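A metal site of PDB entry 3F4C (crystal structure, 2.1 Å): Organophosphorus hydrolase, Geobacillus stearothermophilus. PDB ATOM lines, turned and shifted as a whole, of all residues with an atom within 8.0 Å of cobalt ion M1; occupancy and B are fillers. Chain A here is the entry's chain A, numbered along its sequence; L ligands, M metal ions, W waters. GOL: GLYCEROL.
Cobalt ion M1 is bound by water W1 (2.1 Å), NE2 of His 25 (2.1 Å), NE2 of His 23 (2.2 Å), OD1 of Asp 266 (2.4 Å) and O3 of the ligand (2.4 Å). Slightly farther from cobalt ion M1 lies OQ2 of KCX 145 (2.6 Å).
O of Thr 267 sits at hydrogen-bond distance from N of His 25 (2.8 Å). A ring nitrogen (ND1) of His 25 is in hydrogen-bond range of the side-chain hydroxyl (OG1) of Thr 70. OQ2 of KCX 145 lies close to NE2 of His 23, at 3.2 Å. OD2 of Asp 266 lies within salt-bridge range of NH1 of Arg 230 (2.8 Å). OE1 of Glu 24 lies within hydrogen-bond range of N of Asp 266. N of Asp 266 sits close to O of Asp 229.
Of the 22 residues printed, 4 come within 4 Å of cobalt ion M1. The nearest printed residue that does not touch cobalt ion M1 is His 206 (4.8 Å).
Water W1 bridges OD2 of Asp 266 (2.6 Å) and OQ2 of KCX 145 (3.2 Å).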
ATOM      1  N   HIS A  23      24.879   8.164 -20.401  1.00  0.00           N
ATOM      2  CA  HIS A  23      24.678   6.922 -19.663  1.00  0.00           C
ATOM      3  C   HIS A  23      24.305   7.139 -18.218  1.00  0.00           C
ATOM      4  O   HIS A  23      25.183   7.254 -17.377  1.00  0.00           O
ATOM      5  CB  HIS A  23      25.951   6.048 -19.753  1.00  0.00           C
ATOM      6  CG  HIS A  23      25.774   4.631 -19.302  1.00  0.00           C
ATOM      7  ND1 HIS A  23      26.318   3.554 -19.982  1.00  0.00           N
ATOM      8  CD2 HIS A  23      25.146   4.101 -18.220  1.00  0.00           C
ATOM      9  CE1 HIS A  23      26.034   2.436 -19.345  1.00  0.00           C
ATOM     10  NE2 HIS A  23      25.323   2.738 -18.267  1.00  0.00           N
ATOM     11  N   GLU A  24      23.007   7.190 -17.930  1.00  0.00           N
ATOM     12  CA  GLU A  24      22.550   7.360 -16.544  1.00  0.00           C
ATOM     13  C   GLU A  24      21.331   6.471 -16.375  1.00  0.00           C
ATOM     14  O   GLU A  24      20.628   6.215 -17.347  1.00  0.00           O
ATOM     15  CB  GLU A  24      22.165   8.822 -16.270  1.00  0.00           C
ATOM     16  CG  GLU A  24      23.243   9.867 -16.555  1.00  0.00           C
ATOM     17  CD  GLU A  24      24.484   9.822 -15.632  1.00  0.00           C
ATOM     18  OE1 GLU A  24      24.413   9.289 -14.498  1.00  0.00           O
ATOM     19  OE2 GLU A  24      25.541  10.359 -16.052  1.00  0.00           O
ATOM     20  N   HIS A  25      21.081   5.990 -15.156  1.00  0.00           N
ATOM     21  CA  HIS A  25      19.932   5.146 -14.868  1.00  0.00           C
ATOM     22  C   HIS A  25      18.991   5.815 -13.888  1.00  0.00           C
ATOM     23  O   HIS A  25      19.379   6.124 -12.770  1.00  0.00           O
ATOM     24  CB  HIS A  25      20.352   3.824 -14.227  1.00  0.00           C
ATOM     25  CG  HIS A  25      21.283   3.012 -15.070  1.00  0.00           C
ATOM     26  ND1 HIS A  25      20.836   2.132 -16.046  1.00  0.00           N
ATOM     27  CD2 HIS A  25      22.623   2.956 -15.109  1.00  0.00           C
ATOM     28  CE1 HIS A  25      21.877   1.593 -16.651  1.00  0.00           C
ATOM     29  NE2 HIS A  25      22.969   2.079 -16.094  1.00  0.00           N
ATOM     30  N   PHE A  28      17.148   1.202 -11.579  1.00  0.00           N
ATOM     31  CA  PHE A  28      17.962   0.041 -11.888  1.00  0.00           C
ATOM     32  C   PHE A  28      17.947  -1.081 -10.846  1.00  0.00           C
ATOM     33  O   PHE A  28      17.989  -0.838  -9.643  1.00  0.00           O
ATOM     34  CB  PHE A  28      19.410   0.457 -12.136  1.00  0.00           C
ATOM     35  CG  PHE A  28      20.307  -0.694 -12.484  1.00  0.00           C
ATOM     36  CD1 PHE A  28      20.906  -1.458 -11.494  1.00  0.00           C
ATOM     37  CD2 PHE A  28      20.535  -1.041 -13.832  1.00  0.00           C
ATOM     38  CE1 PHE A  28      21.712  -2.528 -11.827  1.00  0.00           C
ATOM     39  CE2 PHE A  28      21.328  -2.080 -14.160  1.00  0.00           C
ATOM     40  CZ  PHE A  28      21.928  -2.844 -13.147  1.00  0.00           C
ATOM     41  N   VAL A  67      20.545   9.446 -21.942  1.00  0.00           N
ATOM     42  CA  VAL A  67      20.331   8.133 -22.535  1.00  0.00           C
ATOM     43  C   VAL A  67      20.337   7.196 -21.307  1.00  0.00           C
ATOM     44  O   VAL A  67      21.332   7.140 -20.569  1.00  0.00           O
ATOM     45  CB  VAL A  67      21.434   7.731 -23.516  1.00  0.00           C
ATOM     46  CG1 VAL A  67      21.257   6.273 -23.930  1.00  0.00           C
ATOM     47  CG2 VAL A  67      21.367   8.630 -24.782  1.00  0.00           C
ATOM     48  N   ASP A  68      19.212   6.533 -21.060  1.00  0.00           N
ATOM     49  CA  ASP A  68      19.075   5.612 -19.928  1.00  0.00           C
ATOM     50  C   ASP A  68      19.109   4.224 -20.565  1.00  0.00           C
ATOM     51  O   ASP A  68      18.094   3.726 -21.099  1.00  0.00           O
ATOM     52  CB  ASP A  68      17.752   5.853 -19.200  1.00  0.00           C
ATOM     53  CG  ASP A  68      17.592   4.961 -17.991  1.00  0.00           C
ATOM     54  OD1 ASP A  68      18.129   3.840 -18.017  1.00  0.00           O
ATOM     55  OD2 ASP A  68      16.919   5.364 -17.016  1.00  0.00           O
ATOM     56  N   PRO A  69      20.281   3.569 -20.511  1.00  0.00           N
ATOM     57  CA  PRO A  69      20.375   2.259 -21.131  1.00  0.00           C
ATOM     58  C   PRO A  69      20.045   1.047 -20.275  1.00  0.00           C
ATOM     59  O   PRO A  69      20.537  -0.048 -20.518  1.00  0.00           O
ATOM     60  CB  PRO A  69      21.801   2.251 -21.657  1.00  0.00           C
ATOM     61  CG  PRO A  69      22.560   2.962 -20.533  1.00  0.00           C
ATOM     62  CD  PRO A  69      21.582   3.980 -19.938  1.00  0.00           C
ATOM     63  N   THR A  70      19.181   1.234 -19.278  1.00  0.00           N
ATOM     64  CA  THR A  70      18.835   0.112 -18.427  1.00  0.00           C
ATOM     65  C   THR A  70      18.410  -1.101 -19.277  1.00  0.00           C
ATOM     66  O   THR A  70      17.467  -1.016 -20.057  1.00  0.00           O
ATOM     67  CB  THR A  70      17.729   0.514 -17.415  1.00  0.00           C
ATOM     68  OG1 THR A  70      18.208   1.607 -16.597  1.00  0.00           O
ATOM     69  CG2 THR A  70      17.357  -0.679 -16.511  1.00  0.00           C
ATOM     70  N   PRO A  71      19.111  -2.249 -19.132  1.00  0.00           N
ATOM     71  CA  PRO A  71      18.761  -3.456 -19.905  1.00  0.00           C
ATOM     72  C   PRO A  71      17.388  -4.006 -19.537  1.00  0.00           C
ATOM     73  O   PRO A  71      16.892  -3.770 -18.430  1.00  0.00           O
ATOM     74  CB  PRO A  71      19.895  -4.437 -19.566  1.00  0.00           C
ATOM     75  CG  PRO A  71      21.091  -3.487 -19.262  1.00  0.00           C
ATOM     76  CD  PRO A  71      20.389  -2.441 -18.402  1.00  0.00           C
ATOM     77  N   TYR A  99      21.524  -7.615 -19.897  1.00  0.00           N
ATOM     78  CA  TYR A  99      22.824  -7.405 -19.262  1.00  0.00           C
ATOM     79  C   TYR A  99      23.894  -8.490 -19.576  1.00  0.00           C
ATOM     80  O   TYR A  99      23.559  -9.583 -20.078  1.00  0.00           O
ATOM     81  CB  TYR A  99      22.671  -7.223 -17.773  1.00  0.00           C
ATOM     82  CG  TYR A  99      23.689  -6.214 -17.286  1.00  0.00           C
ATOM     83  CD1 TYR A  99      24.327  -5.357 -18.196  1.00  0.00           C
ATOM     84  CD2 TYR A  99      24.030  -6.119 -15.929  1.00  0.00           C
ATOM     85  CE1 TYR A  99      25.290  -4.455 -17.789  1.00  0.00           C
ATOM     86  CE2 TYR A  99      24.989  -5.217 -15.514  1.00  0.00           C
ATOM     87  CZ  TYR A  99      25.625  -4.390 -16.446  1.00  0.00           C
ATOM     88  OH  TYR A  99      26.601  -3.508 -16.045  1.00  0.00           O
ATOM     89  N   KCX A 145      21.352  -1.920 -26.417  1.00  0.00           N
ATOM     90  CA  KCX A 145      22.330  -2.013 -25.348  1.00  0.00           C
ATOM     91  CB  KCX A 145      21.625  -1.747 -24.017  1.00  0.00           C
ATOM     92  CG  KCX A 145      22.518  -1.981 -22.790  1.00  0.00           C
ATOM     93  CD  KCX A 145      23.693  -1.025 -22.782  1.00  0.00           C
ATOM     94  CE  KCX A 145      23.816  -0.527 -21.352  1.00  0.00           C
ATOM     95  NZ  KCX A 145      24.978  -1.076 -20.678  1.00  0.00           N
ATOM     96  C   KCX A 145      23.035  -3.389 -25.303  1.00  0.00           C
ATOM     97  O   KCX A 145      22.384  -4.418 -25.189  1.00  0.00           O
ATOM     98  CX  KCX A 145      25.305  -0.839 -19.402  1.00  0.00           C
ATOM     99  OQ1 KCX A 145      26.359  -1.331 -18.950  1.00  0.00           O
ATOM    100  OQ2 KCX A 145      24.457  -0.350 -18.570  1.00  0.00           O
ATOM    101  N   THR A 177      27.536   0.000 -25.744  1.00  0.00           N
ATOM    102  CA  THR A 177      27.954  -1.223 -25.091  1.00  0.00           C
ATOM    103  C   THR A 177      28.558  -0.923 -23.746  1.00  0.00           C
ATOM    104  O   THR A 177      28.819   0.235 -23.419  1.00  0.00           O
ATOM    105  CB  THR A 177      29.060  -1.939 -25.856  1.00  0.00           C
ATOM    106  OG1 THR A 177      30.302  -1.332 -25.504  1.00  0.00           O
ATOM    107  CG2 THR A 177      28.846  -1.833 -27.362  1.00  0.00           C
ATOM    108  N   HIS A 178      28.799  -1.995 -23.006  1.00  0.00           N
ATOM    109  CA  HIS A 178      29.441  -1.935 -21.713  1.00  0.00           C
ATOM    110  C   HIS A 178      30.583  -2.958 -21.765  1.00  0.00           C
ATOM    111  O   HIS A 178      30.425  -4.033 -22.319  1.00  0.00           O
ATOM    112  CB  HIS A 178      28.407  -2.248 -20.590  1.00  0.00           C
ATOM    113  CG  HIS A 178      28.874  -3.230 -19.562  1.00  0.00           C
ATOM    114  ND1 HIS A 178      28.547  -3.101 -18.228  1.00  0.00           N
ATOM    115  CD2 HIS A 178      29.572  -4.393 -19.660  1.00  0.00           C
ATOM    116  CE1 HIS A 178      29.024  -4.136 -17.547  1.00  0.00           C
ATOM    117  NE2 HIS A 178      29.659  -4.932 -18.391  1.00  0.00           N
ATOM    118  N   HIS A 206      32.295   2.245 -20.611  1.00  0.00           N
ATOM    119  CA  HIS A 206      33.207   1.923 -19.509  1.00  0.00           C
ATOM    120  C   HIS A 206      34.665   1.882 -19.933  1.00  0.00           C
ATOM    121  O   HIS A 206      35.449   1.173 -19.331  1.00  0.00           O
ATOM    122  CB  HIS A 206      32.893   0.585 -18.866  1.00  0.00           C
ATOM    123  CG  HIS A 206      31.529   0.501 -18.292  1.00  0.00           C
ATOM    124  ND1 HIS A 206      30.639   1.560 -18.335  1.00  0.00           N
ATOM    125  CD2 HIS A 206      30.868  -0.529 -17.712  1.00  0.00           C
ATOM    126  CE1 HIS A 206      29.487   1.182 -17.813  1.00  0.00           C
ATOM    127  NE2 HIS A 206      29.596  -0.079 -17.429  1.00  0.00           N
ATOM    128  N   ASP A 229      32.251   6.749 -18.781  1.00  0.00           N
ATOM    129  CA  ASP A 229      30.927   6.934 -18.229  1.00  0.00           C
ATOM    130  C   ASP A 229      30.693   6.488 -16.796  1.00  0.00           C
ATOM    131  O   ASP A 229      29.572   6.223 -16.411  1.00  0.00           O
ATOM    132  CB  ASP A 229      29.904   6.245 -19.175  1.00  0.00           C
ATOM    133  CG  ASP A 229      30.283   4.793 -19.461  1.00  0.00           C
ATOM    134  OD1 ASP A 229      31.009   4.210 -18.620  1.00  0.00           O
ATOM    135  OD2 ASP A 229      29.862   4.224 -20.521  1.00  0.00           O
ATOM    136  N   ARG A 230      31.749   6.420 -15.998  1.00  0.00           N
ATOM    137  CA  ARG A 230      31.569   5.994 -14.638  1.00  0.00           C
ATOM    138  C   ARG A 230      32.241   6.961 -13.671  1.00  0.00           C
ATOM    139  O   ARG A 230      32.694   6.558 -12.599  1.00  0.00           O
ATOM    140  CB  ARG A 230      32.094   4.560 -14.488  1.00  0.00           C
ATOM    141  CG  ARG A 230      31.167   3.512 -15.132  1.00  0.00           C
ATOM    142  CD  ARG A 230      31.798   2.141 -15.240  1.00  0.00           C
ATOM    143  NE  ARG A 230      31.983   1.469 -13.952  1.00  0.00           N
ATOM    144  CZ  ARG A 230      31.027   0.874 -13.246  1.00  0.00           C
ATOM    145  NH1 ARG A 230      29.780   0.869 -13.691  1.00  0.00           N
ATOM    146  NH2 ARG A 230      31.324   0.283 -12.081  1.00  0.00           N
ATOM    147  N   ILE A 233      32.470   6.788  -9.543  1.00  0.00           N
ATOM    148  CA  ILE A 233      32.464   5.436  -9.004  1.00  0.00           C
ATOM    149  C   ILE A 233      33.903   5.022  -8.774  1.00  0.00           C
ATOM    150  O   ILE A 233      34.700   4.895  -9.713  1.00  0.00           O
ATOM    151  CB  ILE A 233      31.853   4.409  -9.989  1.00  0.00           C
ATOM    152  CG1 ILE A 233      30.399   4.755 -10.292  1.00  0.00           C
ATOM    153  CG2 ILE A 233      31.947   3.014  -9.384  1.00  0.00           C
ATOM    154  CD1 ILE A 233      29.799   3.861 -11.391  1.00  0.00           C
ATOM    155  N   HIS A 265      28.179   9.469 -15.743  1.00  0.00           N
ATOM    156  CA  HIS A 265      28.457   8.924 -14.411  1.00  0.00           C
ATOM    157  C   HIS A 265      27.913   7.530 -14.167  1.00  0.00           C
ATOM    158  O   HIS A 265      28.255   6.891 -13.157  1.00  0.00           O
ATOM    159  CB  HIS A 265      27.818   9.764 -13.284  1.00  0.00           C
ATOM    160  CG  HIS A 265      27.906  11.256 -13.457  1.00  0.00           C
ATOM    161  ND1 HIS A 265      27.075  11.962 -14.299  1.00  0.00           N
ATOM    162  CD2 HIS A 265      28.694  12.168 -12.854  1.00  0.00           C
ATOM    163  CE1 HIS A 265      27.346  13.245 -14.207  1.00  0.00           C
ATOM    164  NE2 HIS A 265      28.330  13.406 -13.330  1.00  0.00           N
ATOM    165  N   ASP A 266      27.014   7.076 -15.032  1.00  0.00           N
ATOM    166  CA  ASP A 266      26.415   5.754 -14.833  1.00  0.00           C
ATOM    167  C   ASP A 266      25.718   5.629 -13.470  1.00  0.00           C
ATOM    168  O   ASP A 266      25.791   4.593 -12.815  1.00  0.00           O
ATOM    169  CB  ASP A 266      27.493   4.675 -14.990  1.00  0.00           C
ATOM    170  CG  ASP A 266      26.911   3.278 -15.080  1.00  0.00           C
ATOM    171  OD1 ASP A 266      25.677   3.145 -15.193  1.00  0.00           O
ATOM    172  OD2 ASP A 266      27.710   2.300 -15.021  1.00  0.00           O
ATOM    173  N   THR A 267      25.020   6.684 -13.034  1.00  0.00           N
ATOM    174  CA  THR A 267      24.321   6.661 -11.759  1.00  0.00           C
ATOM    175  C   THR A 267      23.086   5.766 -11.750  1.00  0.00           C
ATOM    176  O   THR A 267      22.538   5.379 -12.786  1.00  0.00           O
ATOM    177  CB  THR A 267      23.861   8.073 -11.344  1.00  0.00           C
ATOM    178  OG1 THR A 267      22.992   8.592 -12.359  1.00  0.00           O
ATOM    179  CG2 THR A 267      25.065   9.035 -11.180  1.00  0.00           C
ATOM    180  N   VAL A 268      22.668   5.419 -10.539  1.00  0.00           N
ATOM    181  CA  VAL A 268      21.490   4.607 -10.306  1.00  0.00           C
ATOM    182  C   VAL A 268      20.810   5.450  -9.263  1.00  0.00           C
ATOM    183  O   VAL A 268      21.181   5.427  -8.103  1.00  0.00           O
ATOM    184  CB  VAL A 268      21.833   3.218  -9.744  1.00  0.00           C
ATOM    185  CG1 VAL A 268      20.569   2.514  -9.286  1.00  0.00           C
ATOM    186  CG2 VAL A 268      22.529   2.386 -10.823  1.00  0.00           C
ATOM    187  N   TRP A 289      29.448  10.105  -6.414  1.00  0.00           N
ATOM    188  CA  TRP A 289      28.715   9.422  -7.471  1.00  0.00           C
ATOM    189  C   TRP A 289      27.278   9.924  -7.579  1.00  0.00           C
ATOM    190  O   TRP A 289      26.380   9.291  -7.078  1.00  0.00           O
ATOM    191  CB  TRP A 289      28.751   7.935  -7.233  1.00  0.00           C
ATOM    192  CG  TRP A 289      28.166   7.120  -8.335  1.00  0.00           C
ATOM    193  CD1 TRP A 289      28.292   7.337  -9.688  1.00  0.00           C
ATOM    194  CD2 TRP A 289      27.419   5.922  -8.189  1.00  0.00           C
ATOM    195  NE1 TRP A 289      27.663   6.334 -10.385  1.00  0.00           N
ATOM    196  CE2 TRP A 289      27.122   5.446  -9.498  1.00  0.00           C
ATOM    197  CE3 TRP A 289      26.967   5.177  -7.075  1.00  0.00           C
ATOM    198  CZ2 TRP A 289      26.390   4.275  -9.728  1.00  0.00           C
ATOM    199  CZ3 TRP A 289      26.235   4.007  -7.305  1.00  0.00           C
ATOM    200  CH2 TRP A 289      25.961   3.570  -8.637  1.00  0.00           C
HETATM  201  C1  GOL L   1      26.781  -2.407 -12.953  1.00  0.00           C
HETATM  202  O1  GOL L   1      27.527  -2.326 -11.843  1.00  0.00           O
HETATM  203  C2  GOL L   1      26.064  -1.108 -13.124  1.00  0.00           C
HETATM  204  O2  GOL L   1      27.048  -0.076 -13.200  1.00  0.00           O
HETATM  205  C3  GOL L   1      25.199  -1.134 -14.407  1.00  0.00           C
HETATM  206  O3  GOL L   1      24.518   0.124 -14.563  1.00  0.00           O
HETATM  207 CO    CO M   1      24.860   1.362 -16.629  1.00  0.00          CO
HETATM  208 CO    CO M   2      27.440  -1.212 -17.089  1.00  0.00          CO
HETATM  209  O   HOH W   1      26.657   0.389 -16.378  1.00  0.00           O
